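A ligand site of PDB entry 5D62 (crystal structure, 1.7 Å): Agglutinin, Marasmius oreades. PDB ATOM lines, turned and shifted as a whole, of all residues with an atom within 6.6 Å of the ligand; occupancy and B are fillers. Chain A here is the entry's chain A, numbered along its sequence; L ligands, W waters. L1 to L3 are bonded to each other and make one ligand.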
ATOM      1  N   HIS A   9      17.241  31.202   4.643  1.00  0.00           N
ATOM      2  CA  HIS A   9      17.244  30.427   3.394  1.00  0.00           C
ATOM      3  C   HIS A   9      18.413  29.453   3.632  1.00  0.00           C
ATOM      4  O   HIS A   9      19.552  29.873   3.872  1.00  0.00           O
ATOM      5  CB  HIS A   9      17.501  31.380   2.259  1.00  0.00           C
ATOM      6  CG  HIS A   9      17.459  30.729   0.922  1.00  0.00           C
ATOM      7  ND1 HIS A   9      18.590  30.397   0.197  1.00  0.00           N
ATOM      8  CD2 HIS A   9      16.403  30.246   0.219  1.00  0.00           C
ATOM      9  CE1 HIS A   9      18.219  29.826  -0.923  1.00  0.00           C
ATOM     10  NE2 HIS A   9      16.901  29.695  -0.930  1.00  0.00           N
ATOM     11  N   ASP A  20      13.647  22.977   0.603  1.00  0.00           N
ATOM     12  CA  ASP A  20      12.459  23.438  -0.093  1.00  0.00           C
ATOM     13  C   ASP A  20      11.247  22.528   0.386  1.00  0.00           C
ATOM     14  O   ASP A  20      11.293  21.320   0.322  1.00  0.00           O
ATOM     15  CB  ASP A  20      12.679  23.299  -1.579  1.00  0.00           C
ATOM     16  CG  ASP A  20      11.516  23.856  -2.476  1.00  0.00           C
ATOM     17  OD1 ASP A  20      10.362  23.285  -2.429  1.00  0.00           O
ATOM     18  OD2 ASP A  20      11.717  24.818  -3.295  1.00  0.00           O
ATOM     19  N   LEU A  21      10.175  23.132   0.779  1.00  0.00           N
ATOM     20  CA  LEU A  21       8.967  22.360   1.151  1.00  0.00           C
ATOM     21  C   LEU A  21       8.198  22.245  -0.163  1.00  0.00           C
ATOM     22  O   LEU A  21       7.736  23.301  -0.731  1.00  0.00           O
ATOM     23  CB  LEU A  21       8.133  23.151   2.155  1.00  0.00           C
ATOM     24  CG  LEU A  21       6.802  22.517   2.521  1.00  0.00           C
ATOM     25  CD1 LEU A  21       6.969  21.157   3.170  1.00  0.00           C
ATOM     26  CD2 LEU A  21       5.972  23.400   3.476  1.00  0.00           C
ATOM     27  N   LYS A  22       8.046  21.044  -0.652  1.00  0.00           N
ATOM     28  CA  LYS A  22       7.561  20.825  -2.043  1.00  0.00           C
ATOM     29  C   LYS A  22       6.196  21.461  -2.288  1.00  0.00           C
ATOM     30  O   LYS A  22       5.216  21.221  -1.571  1.00  0.00           O
ATOM     31  CB  LYS A  22       7.617  19.318  -2.441  1.00  0.00           C
ATOM     32  CG  LYS A  22       7.876  19.164  -3.876  1.00  0.00           C
ATOM     33  CD  LYS A  22       7.844  17.659  -4.248  1.00  0.00           C
ATOM     34  CE  LYS A  22       8.106  17.605  -5.766  1.00  0.00           C
ATOM     35  NZ  LYS A  22       8.378  16.124  -6.097  1.00  0.00           N
ATOM     36  N   ASP A  23       6.149  22.271  -3.354  1.00  0.00           N
ATOM     37  CA  ASP A  23       4.994  23.096  -3.723  1.00  0.00           C
ATOM     38  C   ASP A  23       4.442  24.006  -2.667  1.00  0.00           C
ATOM     39  O   ASP A  23       3.313  24.463  -2.783  1.00  0.00           O
ATOM     40  CB  ASP A  23       3.864  22.180  -4.238  1.00  0.00           C
ATOM     41  CG  ASP A  23       2.974  22.851  -5.290  1.00  0.00           C
ATOM     42  OD1 ASP A  23       3.416  23.645  -6.122  1.00  0.00           O
ATOM     43  OD2 ASP A  23       1.758  22.571  -5.283  1.00  0.00           O
ATOM     44  N   GLY A  24       5.182  24.228  -1.604  1.00  0.00           N
ATOM     45  CA  GLY A  24       4.750  25.041  -0.537  1.00  0.00           C
ATOM     46  C   GLY A  24       3.549  24.449   0.174  1.00  0.00           C
ATOM     47  O   GLY A  24       2.879  25.175   0.898  1.00  0.00           O
ATOM     48  N   VAL A  33      12.727  18.854   0.299  1.00  0.00           N
ATOM     49  CA  VAL A  33      13.555  18.379  -0.779  1.00  0.00           C
ATOM     50  C   VAL A  33      14.603  19.410  -1.074  1.00  0.00           C
ATOM     51  O   VAL A  33      14.432  20.630  -0.768  1.00  0.00           O
ATOM     52  CB  VAL A  33      12.759  18.078  -2.137  1.00  0.00           C
ATOM     53  CG1 VAL A  33      11.840  16.864  -1.986  1.00  0.00           C
ATOM     54  CG2 VAL A  33      11.987  19.270  -2.628  1.00  0.00           C
ATOM     55  N   TRP A  35      16.276  21.837  -3.842  1.00  0.00           N
ATOM     56  CA  TRP A  35      15.782  22.588  -5.025  1.00  0.00           C
ATOM     57  C   TRP A  35      16.673  23.787  -5.303  1.00  0.00           C
ATOM     58  O   TRP A  35      17.093  24.500  -4.405  1.00  0.00           O
ATOM     59  CB  TRP A  35      14.330  23.034  -4.841  1.00  0.00           C
ATOM     60  CG  TRP A  35      13.531  23.174  -6.096  1.00  0.00           C
ATOM     61  CD1 TRP A  35      13.600  24.167  -7.015  1.00  0.00           C
ATOM     62  CD2 TRP A  35      12.600  22.233  -6.597  1.00  0.00           C
ATOM     63  NE1 TRP A  35      12.734  23.925  -8.077  1.00  0.00           N
ATOM     64  CE2 TRP A  35      12.114  22.738  -7.856  1.00  0.00           C
ATOM     65  CE3 TRP A  35      12.122  21.000  -6.113  1.00  0.00           C
ATOM     66  CZ2 TRP A  35      11.176  22.044  -8.647  1.00  0.00           C
ATOM     67  CZ3 TRP A  35      11.203  20.299  -6.913  1.00  0.00           C
ATOM     68  CH2 TRP A  35      10.732  20.838  -8.179  1.00  0.00           C
ATOM     69  N   GLN A  36      16.879  24.111  -6.575  1.00  0.00           N
ATOM     70  CA  GLN A  36      17.613  25.297  -6.947  1.00  0.00           C
ATOM     71  C   GLN A  36      16.884  26.570  -6.611  1.00  0.00           C
ATOM     72  O   GLN A  36      15.692  26.567  -6.386  1.00  0.00           O
ATOM     73  CB  GLN A  36      17.994  25.279  -8.442  1.00  0.00           C
ATOM     74  CG  GLN A  36      16.844  25.483  -9.392  1.00  0.00           C
ATOM     75  CD  GLN A  36      17.271  25.387 -10.858  1.00  0.00           C
ATOM     76  OE1 GLN A  36      17.992  26.233 -11.328  1.00  0.00           O
ATOM     77  NE2 GLN A  36      16.853  24.354 -11.559  1.00  0.00           N
ATOM     78  N   PHE A  37      17.598  27.715  -6.605  1.00  0.00           N
ATOM     79  CA  PHE A  37      17.057  28.966  -6.132  1.00  0.00           C
ATOM     80  C   PHE A  37      17.602  30.114  -6.949  1.00  0.00           C
ATOM     81  O   PHE A  37      18.573  29.895  -7.748  1.00  0.00           O
ATOM     82  CB  PHE A  37      17.392  29.121  -4.605  1.00  0.00           C
ATOM     83  CG  PHE A  37      18.866  29.233  -4.319  1.00  0.00           C
ATOM     84  CD1 PHE A  37      19.592  28.116  -4.029  1.00  0.00           C
ATOM     85  CD2 PHE A  37      19.463  30.456  -4.240  1.00  0.00           C
ATOM     86  CE1 PHE A  37      20.949  28.199  -3.717  1.00  0.00           C
ATOM     87  CE2 PHE A  37      20.867  30.552  -4.018  1.00  0.00           C
ATOM     88  CZ  PHE A  37      21.557  29.401  -3.748  1.00  0.00           C
ATOM     89  N   THR A  38      16.970  31.268  -6.789  1.00  0.00           N
ATOM     90  CA  THR A  38      17.414  32.489  -7.499  1.00  0.00           C
ATOM     91  C   THR A  38      17.808  33.486  -6.403  1.00  0.00           C
ATOM     92  O   THR A  38      16.979  33.824  -5.568  1.00  0.00           O
ATOM     93  CB  THR A  38      16.282  33.038  -8.416  1.00  0.00           C
ATOM     94  OG1 THR A  38      15.838  31.958  -9.284  1.00  0.00           O
ATOM     95  CG2 THR A  38      16.757  34.220  -9.198  1.00  0.00           C
ATOM     96  N   PRO A  39      19.061  33.950  -6.375  1.00  0.00           N
ATOM     97  CA  PRO A  39      19.464  34.993  -5.362  1.00  0.00           C
ATOM     98  C   PRO A  39      18.758  36.303  -5.549  1.00  0.00           C
ATOM     99  O   PRO A  39      18.275  36.572  -6.639  1.00  0.00           O
ATOM    100  CB  PRO A  39      20.966  35.174  -5.582  1.00  0.00           C
ATOM    101  CG  PRO A  39      21.321  34.314  -6.743  1.00  0.00           C
ATOM    102  CD  PRO A  39      20.115  33.673  -7.363  1.00  0.00           C
ATOM    103  N   THR A  41      15.794  37.250  -4.700  1.00  0.00           N
ATOM    104  CA  THR A  41      14.372  37.111  -4.952  1.00  0.00           C
ATOM    105  C   THR A  41      13.775  36.569  -3.636  1.00  0.00           C
ATOM    106  O   THR A  41      14.526  36.066  -2.785  1.00  0.00           O
ATOM    107  CB  THR A  41      14.001  36.049  -5.993  1.00  0.00           C
ATOM    108  OG1 THR A  41      14.374  34.738  -5.532  1.00  0.00           O
ATOM    109  CG2 THR A  41      14.682  36.354  -7.323  1.00  0.00           C
ATOM    110  N   ILE A  42      12.462  36.625  -3.524  1.00  0.00           N
ATOM    111  CA  ILE A  42      11.732  35.806  -2.541  1.00  0.00           C
ATOM    112  C   ILE A  42      11.660  34.381  -3.107  1.00  0.00           C
ATOM    113  O   ILE A  42      10.971  34.152  -4.163  1.00  0.00           O
ATOM    114  CB  ILE A  42      10.327  36.355  -2.259  1.00  0.00           C
ATOM    115  CG1 ILE A  42      10.440  37.774  -1.606  1.00  0.00           C
ATOM    116  CG2 ILE A  42       9.544  35.335  -1.433  1.00  0.00           C
ATOM    117  CD1 ILE A  42      11.155  37.872  -0.280  1.00  0.00           C
ATOM    118  N   ASN A  43      12.315  33.420  -2.426  1.00  0.00           N
ATOM    119  CA  ASN A  43      12.160  31.969  -2.775  1.00  0.00           C
ATOM    120  C   ASN A  43      11.067  31.396  -1.962  1.00  0.00           C
ATOM    121  O   ASN A  43      11.269  31.057  -0.754  1.00  0.00           O
ATOM    122  CB  ASN A  43      13.511  31.240  -2.588  1.00  0.00           C
ATOM    123  CG  ASN A  43      14.537  31.718  -3.617  1.00  0.00           C
ATOM    124  OD1 ASN A  43      14.533  31.255  -4.747  1.00  0.00           O
ATOM    125  ND2 ASN A  43      15.478  32.620  -3.215  1.00  0.00           N
ATOM    126  N   TRP A  44       9.869  31.401  -2.581  1.00  0.00           N
ATOM    127  CA  TRP A  44       8.611  31.305  -1.862  1.00  0.00           C
ATOM    128  C   TRP A  44       8.483  30.052  -1.011  1.00  0.00           C
ATOM    129  O   TRP A  44       7.822  30.074   0.070  1.00  0.00           O
ATOM    130  CB  TRP A  44       7.415  31.341  -2.836  1.00  0.00           C
ATOM    131  CG  TRP A  44       7.132  32.752  -3.235  1.00  0.00           C
ATOM    132  CD1 TRP A  44       7.567  33.394  -4.397  1.00  0.00           C
ATOM    133  CD2 TRP A  44       6.344  33.716  -2.471  1.00  0.00           C
ATOM    134  NE1 TRP A  44       7.126  34.728  -4.352  1.00  0.00           N
ATOM    135  CE2 TRP A  44       6.421  34.953  -3.180  1.00  0.00           C
ATOM    136  CE3 TRP A  44       5.674  33.656  -1.225  1.00  0.00           C
ATOM    137  CZ2 TRP A  44       5.766  36.104  -2.752  1.00  0.00           C
ATOM    138  CZ3 TRP A  44       5.067  34.794  -0.768  1.00  0.00           C
ATOM    139  CH2 TRP A  44       5.095  36.025  -1.550  1.00  0.00           C
ATOM    140  N   HIS A  45       9.060  28.940  -1.461  1.00  0.00           N
ATOM    141  CA  HIS A  45       8.928  27.689  -0.638  1.00  0.00           C
ATOM    142  C   HIS A  45      10.102  27.340   0.215  1.00  0.00           C
ATOM    143  O   HIS A  45      10.168  26.258   0.820  1.00  0.00           O
ATOM    144  CB  HIS A  45       8.541  26.530  -1.543  1.00  0.00           C
ATOM    145  CG  HIS A  45       7.368  26.830  -2.437  1.00  0.00           C
ATOM    146  ND1 HIS A  45       7.193  26.196  -3.647  1.00  0.00           N
ATOM    147  CD2 HIS A  45       6.268  27.570  -2.227  1.00  0.00           C
ATOM    148  CE1 HIS A  45       6.034  26.605  -4.187  1.00  0.00           C
ATOM    149  NE2 HIS A  45       5.445  27.403  -3.331  1.00  0.00           N
ATOM    150  N   GLN A  46      11.106  28.257   0.352  1.00  0.00           N
ATOM    151  CA  GLN A  46      12.441  27.965   0.844  1.00  0.00           C
ATOM    152  C   GLN A  46      12.827  28.837   2.043  1.00  0.00           C
ATOM    153  O   GLN A  46      14.024  28.978   2.319  1.00  0.00           O
ATOM    154  CB  GLN A  46      13.466  28.147  -0.280  1.00  0.00           C
ATOM    155  CG  GLN A  46      13.151  27.192  -1.496  1.00  0.00           C
ATOM    156  CD  GLN A  46      14.142  27.368  -2.631  1.00  0.00           C
ATOM    157  OE1 GLN A  46      15.035  28.258  -2.574  1.00  0.00           O
ATOM    158  NE2 GLN A  46      14.080  26.524  -3.590  1.00  0.00           N
ATOM    159  N   PHE A  66       5.955  30.264   4.243  1.00  0.00           N
ATOM    160  CA  PHE A  66       4.805  30.156   3.384  1.00  0.00           C
ATOM    161  C   PHE A  66       3.715  29.195   3.885  1.00  0.00           C
ATOM    162  O   PHE A  66       2.540  29.630   3.952  1.00  0.00           O
ATOM    163  CB  PHE A  66       5.220  29.712   1.984  1.00  0.00           C
ATOM    164  CG  PHE A  66       4.095  29.665   0.991  1.00  0.00           C
ATOM    165  CD1 PHE A  66       3.559  30.892   0.443  1.00  0.00           C
ATOM    166  CD2 PHE A  66       3.527  28.486   0.568  1.00  0.00           C
ATOM    167  CE1 PHE A  66       2.536  30.878  -0.467  1.00  0.00           C
ATOM    168  CE2 PHE A  66       2.500  28.474  -0.428  1.00  0.00           C
ATOM    169  CZ  PHE A  66       2.005  29.657  -0.922  1.00  0.00           C
ATOM    170  N   ASP A 131      16.534  18.992  -8.814  1.00  0.00           N
ATOM    171  CA  ASP A 131      15.365  19.649  -8.217  1.00  0.00           C
ATOM    172  C   ASP A 131      14.424  18.517  -7.710  1.00  0.00           C
ATOM    173  O   ASP A 131      13.983  17.598  -8.483  1.00  0.00           O
ATOM    174  CB  ASP A 131      14.636  20.565  -9.229  1.00  0.00           C
ATOM    175  CG  ASP A 131      15.422  21.821  -9.530  1.00  0.00           C
ATOM    176  OD1 ASP A 131      16.282  22.120  -8.662  1.00  0.00           O
ATOM    177  OD2 ASP A 131      15.151  22.440 -10.592  1.00  0.00           O
HETATM  178  C1  LIG L   1       8.668  29.325  -8.260  1.00  0.00           C
HETATM  179  C2  LIG L   1       8.375  29.911  -9.646  1.00  0.00           C
HETATM  180  C3  LIG L   1       6.848  29.906  -9.870  1.00  0.00           C
HETATM  181  C4  LIG L   1       6.045  30.568  -8.704  1.00  0.00           C
HETATM  182  C5  LIG L   1       6.410  29.754  -7.417  1.00  0.00           C
HETATM  183  C6  LIG L   1       5.759  30.331  -6.144  1.00  0.00           C
HETATM  184  O1  LIG L   1       9.139  29.146 -10.580  1.00  0.00           O
HETATM  185  O2  LIG L   1       6.649  30.620 -11.111  1.00  0.00           O
HETATM  186  O3  LIG L   1       6.399  31.989  -8.614  1.00  0.00           O
HETATM  187  O4  LIG L   1       7.838  29.839  -7.221  1.00  0.00           O
HETATM  188  C1  LG2 L   2       7.615  25.890  -7.486  1.00  0.00           C
HETATM  189  C2  LG2 L   2       8.576  27.067  -7.180  1.00  0.00           C
HETATM  190  C3  LG2 L   2      10.019  26.633  -7.090  1.00  0.00           C
HETATM  191  C4  LG2 L   2      10.220  25.496  -6.093  1.00  0.00           C
HETATM  192  C5  LG2 L   2       9.102  24.412  -6.375  1.00  0.00           C
HETATM  193  C6  LG2 L   2       9.148  23.261  -5.401  1.00  0.00           C
HETATM  194  O1  LG2 L   2       6.318  26.407  -7.258  1.00  0.00           O
HETATM  195  O2  LG2 L   2       8.408  27.896  -8.378  1.00  0.00           O
HETATM  196  O3  LG2 L   2      10.839  27.793  -6.802  1.00  0.00           O
HETATM  197  O4  LG2 L   2      10.023  26.056  -4.790  1.00  0.00           O
HETATM  198  O5  LG2 L   2       7.740  24.955  -6.415  1.00  0.00           O
HETATM  199  O6  LG2 L   2       8.584  23.552  -4.112  1.00  0.00           O
HETATM  200  C1  LG3 L   3      12.281  27.462  -6.823  1.00  0.00           C
HETATM  201  C2  LG3 L   3      12.955  28.846  -6.622  1.00  0.00           C
HETATM  202  C3  LG3 L   3      12.997  29.714  -7.888  1.00  0.00           C
HETATM  203  C4  LG3 L   3      13.490  28.919  -9.119  1.00  0.00           C
HETATM  204  C5  LG3 L   3      12.540  27.699  -9.201  1.00  0.00           C
HETATM  205  C6  LG3 L   3      12.798  26.774 -10.355  1.00  0.00           C
HETATM  206  O1  LG3 L   3      12.434  29.626  -5.519  1.00  0.00           O
HETATM  207  O2  LG3 L   3      13.865  30.868  -7.665  1.00  0.00           O
HETATM  208  O3  LG3 L   3      14.858  28.489  -8.895  1.00  0.00           O
HETATM  209  O4  LG3 L   3      12.753  26.885  -8.050  1.00  0.00           O
HETATM  210  O5  LG3 L   3      11.949  25.578 -10.391  1.00  0.00           O
HETATM  211  O   HOH W   1      12.418  22.933 -11.858  1.00  0.00           O
HETATM  212  O   HOH W   2       5.859  22.970  -7.159  1.00  0.00           O
HETATM  213  O   HOH W   3       8.835  32.919  -7.802  1.00  0.00           O
HETATM  214  O   HOH W   4      12.438  32.901  -6.619  1.00  0.00           O
HETATM  215  O   HOH W   5       9.312  26.385 -11.029  1.00  0.00           O
HETATM  216  O   HOH W   6      10.148  31.485  -5.587  1.00  0.00           O
HETATM  217  O   HOH W   7      10.654  28.518  -3.699  1.00  0.00           O
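OD1 of Asp 20 lies within hydrogen-bond range of O6 of LG2 L2, 2.5 Å away.
O1 of LG3 L3 sits at hydrogen-bond distance from OD1 of Asn 43.
The backbone NH of Thr 38 is in hydrogen-bond range of an oxygen (O2) of LG3 L3 (3.3 Å).
The side-chain hydroxyl (OG1) of Thr 38 lies within hydrogen-bond range of an oxygen (O2) of LG3 L3 (2.8 Å).
N of Asp 23 lies within hydrogen-bond range of O6 of LG2 L2 (2.9 Å).
NE1 of Trp 35 sits at hydrogen-bond distance from O5 of LG3 L3.
A ring nitrogen (ND1) of His 45 is in hydrogen-bond range of an oxygen (O6) of LG2 L2, 3.0 Å away.
O of Gln 36 sits at hydrogen-bond distance from O3 of LG3 L3 (3.3 Å).
O6 of LG2 L2 lies within hydrogen-bond range of O of Leu 21 (3.5 Å).
The side-chain carboxylate (OD2) of Asp 20 sits at hydrogen-bond distance from the side-chain amide nitrogen (NE2) of Gln 46 (2.9 Å).
O of Val 33 is in hydrogen-bond range of N of Asp 20 (2.8 Å).
The side-chain hydroxyl (OG1) of Thr 41 sits at hydrogen-bond distance from the side-chain amide nitrogen (ND2) of Asn 43, at 3.3 Å.
The backbone carbonyl oxygen (O) of Thr 38 sits at hydrogen-bond distance from the side-chain hydroxyl (OG1) of Thr 41 (2.8 Å).
The backbone carbonyl oxygen (O) of His 45 lies within hydrogen-bond range of the backbone NH (N) of Leu 21, at 3.1 Å.
The backbone NH (N) of Gly 24 lies within hydrogen-bond range of a ring nitrogen (ND1) of His 45 (3.5 Å).
The backbone carbonyl oxygen of Gln 36 lies within hydrogen-bond range of the side-chain amide nitrogen of Gln 46 (3.2 Å).
OE1 of Gln 46 is in hydrogen-bond range of NE2 of His 9 (2.9 Å).
CA of Lys 22 touches O6 of LG2 L2, at 3.6 Å.
Phe 37 touches the ligand.
Trp 44 touches the ligand.
NE2 of Gln 46 touches C1 of LG3 L3, 3.8 Å away.
Hydrophobic or aromatic side chains within 4 Å of the ligand: Trp 35, Trp 44 and His 45.
Within 4 Å of the ligand: Asp 20, Leu 21, Lys 22, Asp 23, Trp 35, Gln 36, Phe 37, Thr 38, Asn 43, Trp 44, His 45 and Gln 46.
The nearest printed residue that does not touch the ligand is Gly 24 (4.3 Å).
Water W4 lies within hydrogen-bond range of an oxygen (O2) of LG3 L3, the side-chain hydroxyl (OG1) of Thr 41, the backbone carbonyl oxygen (O) of Ile 42 and the side-chain amide oxygen (OD1) of Asn 43.
Water W7 lies within hydrogen-bond range of an oxygen (O4) of LG2 L2 (2.8 Å), the backbone NH of His 45 (2.8 Å) and the backbone NH of Trp 44 (3.2 Å).
Water W2 bridges OD1 of Asp 23 (2.7 Å) and O5 of LG2 L2 (2.8 Å).
Water W6 lies within hydrogen-bond range of O1 of LG3 L3, N of Trp 44 and O of Ile 42.
Water W1 lies within hydrogen-bond range of OD2 of Asp 131 and O5 of LG3 L3.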
